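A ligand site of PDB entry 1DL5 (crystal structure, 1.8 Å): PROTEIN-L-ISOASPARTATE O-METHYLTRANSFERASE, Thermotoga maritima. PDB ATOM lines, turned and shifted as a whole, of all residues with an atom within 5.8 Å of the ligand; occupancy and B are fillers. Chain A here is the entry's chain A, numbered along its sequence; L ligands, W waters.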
ATOM      1  N   SER A  48     -34.392 -21.450 -10.029  1.00  0.00           N
ATOM      2  CA  SER A  48     -34.516 -20.913 -11.372  1.00  0.00           C
ATOM      3  C   SER A  48     -34.475 -22.002 -12.436  1.00  0.00           C
ATOM      4  O   SER A  48     -34.879 -21.791 -13.575  1.00  0.00           O
ATOM      5  CB  SER A  48     -33.379 -19.934 -11.641  1.00  0.00           C
ATOM      6  OG  SER A  48     -32.135 -20.574 -11.426  1.00  0.00           O
ATOM      7  N   TYR A  55     -29.600 -28.382 -11.191  1.00  0.00           N
ATOM      8  CA  TYR A  55     -30.348 -27.423 -10.393  1.00  0.00           C
ATOM      9  C   TYR A  55     -29.622 -26.087 -10.288  1.00  0.00           C
ATOM     10  O   TYR A  55     -28.404 -26.031 -10.261  1.00  0.00           O
ATOM     11  CB  TYR A  55     -30.515 -28.072  -9.006  1.00  0.00           C
ATOM     12  CG  TYR A  55     -31.088 -27.231  -7.907  1.00  0.00           C
ATOM     13  CD1 TYR A  55     -32.456 -26.982  -7.837  1.00  0.00           C
ATOM     14  CD2 TYR A  55     -30.269 -26.743  -6.881  1.00  0.00           C
ATOM     15  CE1 TYR A  55     -33.009 -26.284  -6.757  1.00  0.00           C
ATOM     16  CE2 TYR A  55     -30.808 -26.048  -5.804  1.00  0.00           C
ATOM     17  CZ  TYR A  55     -32.175 -25.822  -5.742  1.00  0.00           C
ATOM     18  OH  TYR A  55     -32.720 -25.156  -4.670  1.00  0.00           O
ATOM     19  N   SER A  56     -30.389 -25.000 -10.255  1.00  0.00           N
ATOM     20  CA  SER A  56     -29.806 -23.671 -10.099  1.00  0.00           C
ATOM     21  C   SER A  56     -30.794 -22.766  -9.384  1.00  0.00           C
ATOM     22  O   SER A  56     -31.998 -22.968  -9.459  1.00  0.00           O
ATOM     23  CB  SER A  56     -29.451 -23.050 -11.452  1.00  0.00           C
ATOM     24  OG  SER A  56     -28.677 -21.871 -11.257  1.00  0.00           O
ATOM     25  N   THR A  57     -30.270 -21.777  -8.675  1.00  0.00           N
ATOM     26  CA  THR A  57     -31.116 -20.859  -7.939  1.00  0.00           C
ATOM     27  C   THR A  57     -30.750 -19.401  -8.136  1.00  0.00           C
ATOM     28  O   THR A  57     -29.593 -19.060  -8.401  1.00  0.00           O
ATOM     29  CB  THR A  57     -31.072 -21.145  -6.417  1.00  0.00           C
ATOM     30  OG1 THR A  57     -29.726 -21.017  -5.943  1.00  0.00           O
ATOM     31  CG2 THR A  57     -31.569 -22.555  -6.126  1.00  0.00           C
ATOM     32  N   SER A  58     -31.754 -18.524  -8.041  1.00  0.00           N
ATOM     33  CA  SER A  58     -31.511 -17.089  -8.127  1.00  0.00           C
ATOM     34  C   SER A  58     -31.337 -16.687  -6.669  1.00  0.00           C
ATOM     35  O   SER A  58     -32.220 -16.958  -5.851  1.00  0.00           O
ATOM     36  CB  SER A  58     -32.721 -16.349  -8.710  1.00  0.00           C
ATOM     37  OG  SER A  58     -32.562 -14.954  -8.548  1.00  0.00           O
ATOM     38  N   SER A  59     -30.208 -16.051  -6.356  1.00  0.00           N
ATOM     39  CA  SER A  59     -29.882 -15.656  -4.992  1.00  0.00           C
ATOM     40  C   SER A  59     -30.765 -14.571  -4.371  1.00  0.00           C
ATOM     41  O   SER A  59     -31.454 -13.843  -5.078  1.00  0.00           O
ATOM     42  CB  SER A  59     -28.420 -15.182  -4.941  1.00  0.00           C
ATOM     43  OG  SER A  59     -27.559 -16.139  -5.509  1.00  0.00           O
ATOM     44  N   MET A  64     -27.227  -9.990  -2.609  1.00  0.00           N
ATOM     45  CA  MET A  64     -26.497  -9.580  -3.799  1.00  0.00           C
ATOM     46  C   MET A  64     -26.265  -8.075  -3.776  1.00  0.00           C
ATOM     47  O   MET A  64     -25.203  -7.596  -4.158  1.00  0.00           O
ATOM     48  CB  MET A  64     -27.258  -9.985  -5.061  1.00  0.00           C
ATOM     49  CG  MET A  64     -27.290 -11.494  -5.285  1.00  0.00           C
ATOM     50  SD  MET A  64     -25.635 -12.217  -5.490  1.00  0.00           S
ATOM     51  CE  MET A  64     -25.283 -12.800  -3.807  1.00  0.00           C
ATOM     52  N   GLU A  81     -18.040 -12.627 -12.889  1.00  0.00           N
ATOM     53  CA  GLU A  81     -18.919 -13.334 -11.953  1.00  0.00           C
ATOM     54  C   GLU A  81     -18.691 -14.836 -12.095  1.00  0.00           C
ATOM     55  O   GLU A  81     -18.589 -15.348 -13.209  1.00  0.00           O
ATOM     56  CB  GLU A  81     -20.395 -13.015 -12.239  1.00  0.00           C
ATOM     57  CG  GLU A  81     -21.349 -13.728 -11.272  1.00  0.00           C
ATOM     58  CD  GLU A  81     -22.808 -13.538 -11.630  1.00  0.00           C
ATOM     59  OE1 GLU A  81     -23.173 -13.778 -12.794  1.00  0.00           O
ATOM     60  OE2 GLU A  81     -23.592 -13.166 -10.735  1.00  0.00           O
ATOM     61  N   ILE A  82     -18.585 -15.530 -10.968  1.00  0.00           N
ATOM     62  CA  ILE A  82     -18.359 -16.970 -10.960  1.00  0.00           C
ATOM     63  C   ILE A  82     -19.633 -17.669 -10.469  1.00  0.00           C
ATOM     64  O   ILE A  82     -20.037 -17.472  -9.324  1.00  0.00           O
ATOM     65  CB  ILE A  82     -17.188 -17.333 -10.017  1.00  0.00           C
ATOM     66  CG1 ILE A  82     -15.921 -16.615 -10.487  1.00  0.00           C
ATOM     67  CG2 ILE A  82     -16.985 -18.852  -9.982  1.00  0.00           C
ATOM     68  CD1 ILE A  82     -15.470 -16.980 -11.906  1.00  0.00           C
ATOM     69  N   GLY A  83     -20.246 -18.463 -11.346  1.00  0.00           N
ATOM     70  CA  GLY A  83     -21.481 -19.172 -11.012  1.00  0.00           C
ATOM     71  C   GLY A  83     -22.683 -18.372 -11.489  1.00  0.00           C
ATOM     72  O   GLY A  83     -23.566 -18.025 -10.700  1.00  0.00           O
ATOM     73  N   GLY A  84     -22.717 -18.094 -12.792  1.00  0.00           N
ATOM     74  CA  GLY A  84     -23.771 -17.301 -13.405  1.00  0.00           C
ATOM     75  C   GLY A  84     -25.215 -17.744 -13.381  1.00  0.00           C
ATOM     76  O   GLY A  84     -26.112 -16.900 -13.479  1.00  0.00           O
ATOM     77  N   GLY A  85     -25.460 -19.046 -13.280  1.00  0.00           N
ATOM     78  CA  GLY A  85     -26.835 -19.539 -13.238  1.00  0.00           C
ATOM     79  C   GLY A  85     -27.585 -19.125 -14.484  1.00  0.00           C
ATOM     80  O   GLY A  85     -27.009 -19.103 -15.569  1.00  0.00           O
ATOM     81  N   THR A  86     -28.879 -18.803 -14.350  1.00  0.00           N
ATOM     82  CA  THR A  86     -29.661 -18.392 -15.513  1.00  0.00           C
ATOM     83  C   THR A  86     -29.465 -16.922 -15.863  1.00  0.00           C
ATOM     84  O   THR A  86     -30.090 -16.415 -16.800  1.00  0.00           O
ATOM     85  CB  THR A  86     -31.163 -18.702 -15.344  1.00  0.00           C
ATOM     86  OG1 THR A  86     -31.661 -18.046 -14.169  1.00  0.00           O
ATOM     87  CG2 THR A  86     -31.377 -20.206 -15.214  1.00  0.00           C
ATOM     88  N   GLY A  87     -28.623 -16.227 -15.090  1.00  0.00           N
ATOM     89  CA  GLY A  87     -28.293 -14.849 -15.403  1.00  0.00           C
ATOM     90  C   GLY A  87     -28.866 -13.634 -14.709  1.00  0.00           C
ATOM     91  O   GLY A  87     -28.469 -12.514 -15.039  1.00  0.00           O
ATOM     92  N   TYR A  88     -29.789 -13.806 -13.768  1.00  0.00           N
ATOM     93  CA  TYR A  88     -30.381 -12.652 -13.102  1.00  0.00           C
ATOM     94  C   TYR A  88     -29.379 -11.711 -12.458  1.00  0.00           C
ATOM     95  O   TYR A  88     -29.413 -10.511 -12.709  1.00  0.00           O
ATOM     96  CB  TYR A  88     -31.414 -13.082 -12.065  1.00  0.00           C
ATOM     97  CG  TYR A  88     -32.034 -11.930 -11.307  1.00  0.00           C
ATOM     98  CD1 TYR A  88     -32.754 -10.932 -11.977  1.00  0.00           C
ATOM     99  CD2 TYR A  88     -31.920 -11.850  -9.915  1.00  0.00           C
ATOM    100  CE1 TYR A  88     -33.359  -9.876 -11.263  1.00  0.00           C
ATOM    101  CE2 TYR A  88     -32.513 -10.810  -9.203  1.00  0.00           C
ATOM    102  CZ  TYR A  88     -33.240  -9.840  -9.878  1.00  0.00           C
ATOM    103  OH  TYR A  88     -33.834  -8.827  -9.151  1.00  0.00           O
ATOM    104  N   ASN A  89     -28.479 -12.223 -11.630  1.00  0.00           N
ATOM    105  CA  ASN A  89     -27.522 -11.339 -10.977  1.00  0.00           C
ATOM    106  C   ASN A  89     -26.586 -10.649 -11.968  1.00  0.00           C
ATOM    107  O   ASN A  89     -26.252  -9.474 -11.805  1.00  0.00           O
ATOM    108  CB  ASN A  89     -26.696 -12.080  -9.930  1.00  0.00           C
ATOM    109  CG  ASN A  89     -25.941 -11.125  -9.020  1.00  0.00           C
ATOM    110  OD1 ASN A  89     -26.556 -10.322  -8.313  1.00  0.00           O
ATOM    111  ND2 ASN A  89     -24.609 -11.207  -9.028  1.00  0.00           N
ATOM    112  N   ALA A  90     -26.182 -11.370 -13.003  1.00  0.00           N
ATOM    113  CA  ALA A  90     -25.302 -10.792 -14.016  1.00  0.00           C
ATOM    114  C   ALA A  90     -26.036  -9.632 -14.682  1.00  0.00           C
ATOM    115  O   ALA A  90     -25.453  -8.558 -14.923  1.00  0.00           O
ATOM    116  CB  ALA A  90     -24.926 -11.865 -15.061  1.00  0.00           C
ATOM    117  N   VAL A 106     -19.394 -16.809 -15.630  1.00  0.00           N
ATOM    118  CA  VAL A 106     -19.104 -18.204 -15.950  1.00  0.00           C
ATOM    119  C   VAL A 106     -20.097 -19.169 -15.305  1.00  0.00           C
ATOM    120  O   VAL A 106     -20.357 -19.084 -14.102  1.00  0.00           O
ATOM    121  CB  VAL A 106     -17.679 -18.587 -15.474  1.00  0.00           C
ATOM    122  CG1 VAL A 106     -17.306 -19.969 -15.997  1.00  0.00           C
ATOM    123  CG2 VAL A 106     -16.673 -17.538 -15.955  1.00  0.00           C
ATOM    124  N   GLU A 107     -20.658 -20.067 -16.110  1.00  0.00           N
ATOM    125  CA  GLU A 107     -21.599 -21.070 -15.611  1.00  0.00           C
ATOM    126  C   GLU A 107     -21.125 -22.432 -16.101  1.00  0.00           C
ATOM    127  O   GLU A 107     -20.955 -22.643 -17.305  1.00  0.00           O
ATOM    128  CB  GLU A 107     -23.021 -20.795 -16.115  1.00  0.00           C
ATOM    129  CG  GLU A 107     -24.027 -21.925 -15.864  1.00  0.00           C
ATOM    130  CD  GLU A 107     -24.097 -22.374 -14.415  1.00  0.00           C
ATOM    131  OE1 GLU A 107     -24.306 -21.529 -13.513  1.00  0.00           O
ATOM    132  OE2 GLU A 107     -23.962 -23.601 -14.158  1.00  0.00           O
ATOM    133  N   TYR A 108     -20.928 -23.343 -15.160  1.00  0.00           N
ATOM    134  CA  TYR A 108     -20.420 -24.699 -15.409  1.00  0.00           C
ATOM    135  C   TYR A 108     -21.384 -25.617 -16.150  1.00  0.00           C
ATOM    136  O   TYR A 108     -20.956 -26.448 -16.958  1.00  0.00           O
ATOM    137  CB  TYR A 108     -20.013 -25.317 -14.062  1.00  0.00           C
ATOM    138  CG  TYR A 108     -19.183 -26.577 -14.132  1.00  0.00           C
ATOM    139  CD1 TYR A 108     -18.134 -26.699 -15.039  1.00  0.00           C
ATOM    140  CD2 TYR A 108     -19.406 -27.626 -13.232  1.00  0.00           C
ATOM    141  CE1 TYR A 108     -17.318 -27.839 -15.048  1.00  0.00           C
ATOM    142  CE2 TYR A 108     -18.593 -28.756 -13.231  1.00  0.00           C
ATOM    143  CZ  TYR A 108     -17.557 -28.849 -14.149  1.00  0.00           C
ATOM    144  OH  TYR A 108     -16.747 -29.970 -14.137  1.00  0.00           O
ATOM    145  N   SER A 109     -22.670 -25.510 -15.865  1.00  0.00           N
ATOM    146  CA  SER A 109     -23.659 -26.342 -16.537  1.00  0.00           C
ATOM    147  C   SER A 109     -23.916 -25.834 -17.944  1.00  0.00           C
ATOM    148  O   SER A 109     -24.242 -24.663 -18.129  1.00  0.00           O
ATOM    149  CB  SER A 109     -24.977 -26.355 -15.746  1.00  0.00           C
ATOM    150  OG  SER A 109     -26.021 -26.896 -16.544  1.00  0.00           O
ATOM    151  N   ILE A 112     -27.737 -24.817 -18.352  1.00  0.00           N
ATOM    152  CA  ILE A 112     -28.054 -23.594 -17.615  1.00  0.00           C
ATOM    153  C   ILE A 112     -27.369 -22.383 -18.247  1.00  0.00           C
ATOM    154  O   ILE A 112     -27.955 -21.305 -18.337  1.00  0.00           O
ATOM    155  CB  ILE A 112     -27.667 -23.744 -16.124  1.00  0.00           C
ATOM    156  CG1 ILE A 112     -28.538 -24.819 -15.478  1.00  0.00           C
ATOM    157  CG2 ILE A 112     -27.824 -22.406 -15.394  1.00  0.00           C
ATOM    158  CD1 ILE A 112     -28.085 -25.258 -14.104  1.00  0.00           C
ATOM    159  N   GLY A 133     -18.278 -23.001 -18.775  1.00  0.00           N
ATOM    160  CA  GLY A 133     -17.127 -23.795 -18.388  1.00  0.00           C
ATOM    161  C   GLY A 133     -16.881 -23.714 -16.887  1.00  0.00           C
ATOM    162  O   GLY A 133     -17.681 -23.143 -16.161  1.00  0.00           O
ATOM    163  N   ASP A 134     -15.774 -24.297 -16.443  1.00  0.00           N
ATOM    164  CA  ASP A 134     -15.404 -24.306 -15.028  1.00  0.00           C
ATOM    165  C   ASP A 134     -14.854 -22.932 -14.628  1.00  0.00           C
ATOM    166  O   ASP A 134     -13.845 -22.480 -15.168  1.00  0.00           O
ATOM    167  CB  ASP A 134     -14.315 -25.354 -14.790  1.00  0.00           C
ATOM    168  CG  ASP A 134     -14.106 -25.679 -13.320  1.00  0.00           C
ATOM    169  OD1 ASP A 134     -14.485 -24.854 -12.462  1.00  0.00           O
ATOM    170  OD2 ASP A 134     -13.548 -26.754 -13.024  1.00  0.00           O
ATOM    171  N   GLY A 135     -15.532 -22.290 -13.682  1.00  0.00           N
ATOM    172  CA  GLY A 135     -15.104 -20.983 -13.218  1.00  0.00           C
ATOM    173  C   GLY A 135     -13.671 -20.968 -12.702  1.00  0.00           C
ATOM    174  O   GLY A 135     -13.044 -19.911 -12.617  1.00  0.00           O
ATOM    175  N   TYR A 136     -13.156 -22.139 -12.360  1.00  0.00           N
ATOM    176  CA  TYR A 136     -11.777 -22.260 -11.874  1.00  0.00           C
ATOM    177  C   TYR A 136     -10.782 -21.520 -12.783  1.00  0.00           C
ATOM    178  O   TYR A 136      -9.846 -20.861 -12.315  1.00  0.00           O
ATOM    179  CB  TYR A 136     -11.370 -23.735 -11.797  1.00  0.00           C
ATOM    180  CG  TYR A 136      -9.930 -23.918 -11.372  1.00  0.00           C
ATOM    181  CD1 TYR A 136      -9.570 -23.929 -10.027  1.00  0.00           C
ATOM    182  CD2 TYR A 136      -8.917 -24.013 -12.325  1.00  0.00           C
ATOM    183  CE1 TYR A 136      -8.229 -24.009  -9.630  1.00  0.00           C
ATOM    184  CE2 TYR A 136      -7.566 -24.096 -11.940  1.00  0.00           C
ATOM    185  CZ  TYR A 136      -7.242 -24.096 -10.597  1.00  0.00           C
ATOM    186  OH  TYR A 136      -5.921 -24.163 -10.227  1.00  0.00           O
ATOM    187  N   THR A 151     -20.754 -16.196  -6.786  1.00  0.00           N
ATOM    188  CA  THR A 151     -22.087 -16.553  -6.333  1.00  0.00           C
ATOM    189  C   THR A 151     -22.313 -18.063  -6.242  1.00  0.00           C
ATOM    190  O   THR A 151     -23.393 -18.567  -6.543  1.00  0.00           O
ATOM    191  CB  THR A 151     -23.158 -15.934  -7.264  1.00  0.00           C
ATOM    192  OG1 THR A 151     -22.964 -16.389  -8.610  1.00  0.00           O
ATOM    193  CG2 THR A 151     -23.047 -14.415  -7.262  1.00  0.00           C
ATOM    194  N   VAL A 152     -21.266 -18.772  -5.827  1.00  0.00           N
ATOM    195  CA  VAL A 152     -21.309 -20.220  -5.648  1.00  0.00           C
ATOM    196  C   VAL A 152     -20.214 -20.508  -4.621  1.00  0.00           C
ATOM    197  O   VAL A 152     -19.192 -19.827  -4.609  1.00  0.00           O
ATOM    198  CB  VAL A 152     -21.055 -20.977  -6.982  1.00  0.00           C
ATOM    199  CG1 VAL A 152     -19.664 -20.658  -7.530  1.00  0.00           C
ATOM    200  CG2 VAL A 152     -21.229 -22.482  -6.781  1.00  0.00           C
ATOM    201  N   ILE A 206     -25.004 -22.554  -3.376  1.00  0.00           N
ATOM    202  CA  ILE A 206     -24.859 -23.919  -3.847  1.00  0.00           C
ATOM    203  C   ILE A 206     -23.346 -24.170  -3.811  1.00  0.00           C
ATOM    204  O   ILE A 206     -22.572 -23.252  -4.095  1.00  0.00           O
ATOM    205  CB  ILE A 206     -25.362 -24.038  -5.313  1.00  0.00           C
ATOM    206  CG1 ILE A 206     -26.880 -23.852  -5.350  1.00  0.00           C
ATOM    207  CG2 ILE A 206     -24.931 -25.375  -5.900  1.00  0.00           C
ATOM    208  CD1 ILE A 206     -27.479 -23.834  -6.765  1.00  0.00           C
ATOM    209  N   THR A 207     -22.933 -25.376  -3.467  1.00  0.00           N
ATOM    210  CA  THR A 207     -21.504 -25.701  -3.419  1.00  0.00           C
ATOM    211  C   THR A 207     -21.011 -25.999  -4.837  1.00  0.00           C
ATOM    212  O   THR A 207     -21.652 -26.749  -5.565  1.00  0.00           O
ATOM    213  CB  THR A 207     -21.228 -26.910  -2.513  1.00  0.00           C
ATOM    214  OG1 THR A 207     -21.699 -26.616  -1.183  1.00  0.00           O
ATOM    215  CG2 THR A 207     -19.737 -27.228  -2.461  1.00  0.00           C
ATOM    216  N   ALA A 208     -19.883 -25.412  -5.210  1.00  0.00           N
ATOM    217  CA  ALA A 208     -19.327 -25.584  -6.558  1.00  0.00           C
ATOM    218  C   ALA A 208     -18.879 -26.986  -6.921  1.00  0.00           C
ATOM    219  O   ALA A 208     -18.467 -27.774  -6.066  1.00  0.00           O
ATOM    220  CB  ALA A 208     -18.157 -24.621  -6.771  1.00  0.00           C
ATOM    221  N   GLY A 209     -18.961 -27.285  -8.209  1.00  0.00           N
ATOM    222  CA  GLY A 209     -18.516 -28.568  -8.723  1.00  0.00           C
ATOM    223  C   GLY A 209     -17.216 -28.275  -9.461  1.00  0.00           C
ATOM    224  O   GLY A 209     -16.663 -27.187  -9.339  1.00  0.00           O
ATOM    225  N   GLY A 210     -16.724 -29.247 -10.238  1.00  0.00           N
ATOM    226  CA  GLY A 210     -15.494 -29.031 -10.968  1.00  0.00           C
ATOM    227  C   GLY A 210     -14.284 -28.771 -10.075  1.00  0.00           C
ATOM    228  O   GLY A 210     -14.233 -29.223  -8.932  1.00  0.00           O
ATOM    229  N   ASN A 211     -13.309 -28.037 -10.601  1.00  0.00           N
ATOM    230  CA  ASN A 211     -12.094 -27.739  -9.861  1.00  0.00           C
ATOM    231  C   ASN A 211     -12.310 -26.730  -8.727  1.00  0.00           C
ATOM    232  O   ASN A 211     -11.375 -26.397  -8.007  1.00  0.00           O
ATOM    233  CB  ASN A 211     -11.003 -27.236 -10.808  1.00  0.00           C
ATOM    234  CG  ASN A 211     -10.417 -28.357 -11.665  1.00  0.00           C
ATOM    235  OD1 ASN A 211     -10.087 -28.149 -12.832  1.00  0.00           O
ATOM    236  ND2 ASN A 211     -10.255 -29.539 -11.076  1.00  0.00           N
ATOM    237  N   LEU A 212     -13.539 -26.228  -8.583  1.00  0.00           N
ATOM    238  CA  LEU A 212     -13.805 -25.288  -7.510  1.00  0.00           C
ATOM    239  C   LEU A 212     -14.379 -26.042  -6.308  1.00  0.00           C
ATOM    240  O   LEU A 212     -14.712 -25.442  -5.288  1.00  0.00           O
ATOM    241  CB  LEU A 212     -14.780 -24.191  -7.974  1.00  0.00           C
ATOM    242  CG  LEU A 212     -14.149 -23.179  -8.932  1.00  0.00           C
ATOM    243  CD1 LEU A 212     -15.188 -22.131  -9.351  1.00  0.00           C
ATOM    244  CD2 LEU A 212     -12.955 -22.498  -8.256  1.00  0.00           C
HETATM  245  N1  LIG L   1     -25.502 -15.511  -9.926  1.00  0.00           N
HETATM  246  C1  LIG L   1     -26.409 -16.795 -10.164  1.00  0.00           C
HETATM  247  C2  LIG L   1     -26.365 -17.701  -8.929  1.00  0.00           C
HETATM  248  C3  LIG L   1     -26.605 -19.111  -9.684  1.00  0.00           C
HETATM  249  S1  LIG L   1     -26.538 -20.475  -8.532  1.00  0.00           S
HETATM  250  C4  LIG L   1     -27.831 -16.139 -10.645  1.00  0.00           C
HETATM  251  O1  LIG L   1     -28.024 -14.937 -10.621  1.00  0.00           O
HETATM  252  O2  LIG L   1     -28.706 -16.996 -10.854  1.00  0.00           O
HETATM  253  C5  LIG L   1     -24.776 -20.756  -8.687  1.00  0.00           C
HETATM  254  C6  LIG L   1     -24.315 -21.704  -9.950  1.00  0.00           C
HETATM  255  O3  LIG L   1     -22.892 -21.873  -9.888  1.00  0.00           O
HETATM  256  C7  LIG L   1     -25.269 -22.914 -10.478  1.00  0.00           C
HETATM  257  O4  LIG L   1     -25.879 -22.499 -11.522  1.00  0.00           O
HETATM  258  C8  LIG L   1     -24.166 -23.867 -10.738  1.00  0.00           C
HETATM  259  O5  LIG L   1     -24.200 -24.842 -11.743  1.00  0.00           O
HETATM  260  C9  LIG L   1     -22.776 -22.923 -10.748  1.00  0.00           C
HETATM  261  N2  LIG L   1     -21.567 -23.694 -10.611  1.00  0.00           N
HETATM  262  C10 LIG L   1     -21.124 -24.701  -9.831  1.00  0.00           C
HETATM  263  N3  LIG L   1     -19.962 -25.155  -9.952  1.00  0.00           N
HETATM  264  C11 LIG L   1     -19.483 -24.353 -10.693  1.00  0.00           C
HETATM  265  C12 LIG L   1     -17.945 -24.135 -11.290  1.00  0.00           C
HETATM  266  N4  LIG L   1     -16.962 -24.829 -11.047  1.00  0.00           N
HETATM  267  N5  LIG L   1     -17.875 -22.935 -12.229  1.00  0.00           N
HETATM  268  C13 LIG L   1     -18.738 -21.985 -12.789  1.00  0.00           C
HETATM  269  N6  LIG L   1     -20.107 -22.237 -12.257  1.00  0.00           N
HETATM  270  C14 LIG L   1     -20.517 -23.409 -11.163  1.00  0.00           C
HETATM  271  O   HOH W   1     -25.823 -14.249 -12.710  1.00  0.00           O
HETATM  272  O   HOH W   2     -22.875 -27.131 -12.457  1.00  0.00           O
HETATM  273  O   HOH W   3     -29.976 -14.488  -8.843  1.00  0.00           O
HETATM  274  O   HOH W   4     -30.825 -16.223 -12.368  1.00  0.00           O
HETATM  275  O   HOH W   5     -25.385 -20.346  -5.355  1.00  0.00           O
HETATM  276  O   HOH W   6     -29.759 -19.428 -11.635  1.00  0.00           O
HETATM  277  O   HOH W   7     -26.416 -14.607  -7.431  1.00  0.00           O
HETATM  278  O   HOH W   8     -22.596 -26.940  -8.028  1.00  0.00           O
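O of Glu 107 lies within hydrogen-bond range of N of Gly 133, at 3.1 Å. The backbone NH (N) of Tyr 136 lies close to the side-chain carboxylate (OD1) of Asp 134, at 3.0 Å. The backbone NH of Asn 211 sits at hydrogen-bond distance from the side-chain carboxylate of Asp 134. The backbone carbonyl oxygen (O) of Ser 56 sits at hydrogen-bond distance from the backbone NH (N) of Ser 48 (2.9 Å). The backbone NH of Thr 151 lies within hydrogen-bond range of the backbone carbonyl oxygen of Ile 82 (2.9 Å). The backbone NH (N) of Val 106 sits at hydrogen-bond distance from the backbone carbonyl oxygen (O) of Glu 81 (2.9 Å). O of Val 106 lies within hydrogen-bond range of N of Gly 83 (2.8 Å). O of Val 106 is in hydrogen-bond range of N of Gly 84 (2.9 Å).
Water W3 lies within hydrogen-bond range of OG of Ser 58, O1 of the ligand and N of Ser 59. Water W4 lies within hydrogen-bond range of the side-chain hydroxyl of Thr 86 (2.7 Å), an oxygen (O2) of the ligand (2.7 Å) and the backbone NH of Tyr 88 (3.0 Å). Water W6 lies within hydrogen-bond range of OG of Ser 48 (2.6 Å), OG of Ser 56 (2.7 Å), O2 of the ligand (2.8 Å), N of Thr 86 (2.9 Å) and O of Thr 57 (3.3 Å). Water W7 lies within hydrogen-bond range of OG of Ser 59 (2.7 Å), N1 of the ligand (2.8 Å) and SD of Met 64 (3.2 Å). Water W1 lies within hydrogen-bond range of the side-chain carboxylate (OE1) of Glu 81 (2.7 Å), the backbone carbonyl oxygen (O) of Gly 84 (2.8 Å), the backbone NH (N) of Ala 90 (2.9 Å) and a nitrogen (N1) of the ligand (3.1 Å). Water W5 lies within hydrogen-bond range of O of Thr 151 (2.9 Å), N of Ile 206 (3.0 Å) and S1 of the ligand (3.4 Å).
The side-chain carboxylate (OE1) of Glu 107 is in hydrogen-bond range of an oxygen (O4) of the ligand. N of Gly 135 is in hydrogen-bond range of N5 of the ligand (2.8 Å). OD1 of Asp 134 sits at hydrogen-bond distance from N4 of the ligand, at 2.9 Å. The side-chain hydroxyl (OG) of Ser 56 sits at hydrogen-bond distance from an oxygen (O4) of the ligand (2.9 Å). The backbone NH of Gly 209 is in hydrogen-bond range of a nitrogen (N3) of the ligand (2.9 Å). O of Gly 209 is in hydrogen-bond range of N4 of the ligand, 2.9 Å away. N of Asn 89 sits at hydrogen-bond distance from O1 of the ligand. The side-chain hydroxyl (OG1) of Thr 151 lies within hydrogen-bond range of a nitrogen (N1) of the ligand (3.0 Å). N1 of the ligand is in salt-bridge range of OE2 of Glu 81 (3.1 Å). O of Gly 83 sits close to N1 of the ligand, at 3.3 Å. N6 of the ligand lies within hydrogen-bond range of N of Tyr 108 (3.2 Å).
The backbone carbonyl oxygen (O) of Thr 57 sits close to an oxygen (O2) of the ligand. Merely in contact with the ligand: Ser 58, Ser 59, Gly 84, Gly 85, Thr 86, Tyr 88, Val 106, Gly 133, Val 152, Ile 206, Ala 208 and Leu 212. The nearest printed residue that does not touch the ligand is Gly 87 (4.3 Å).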
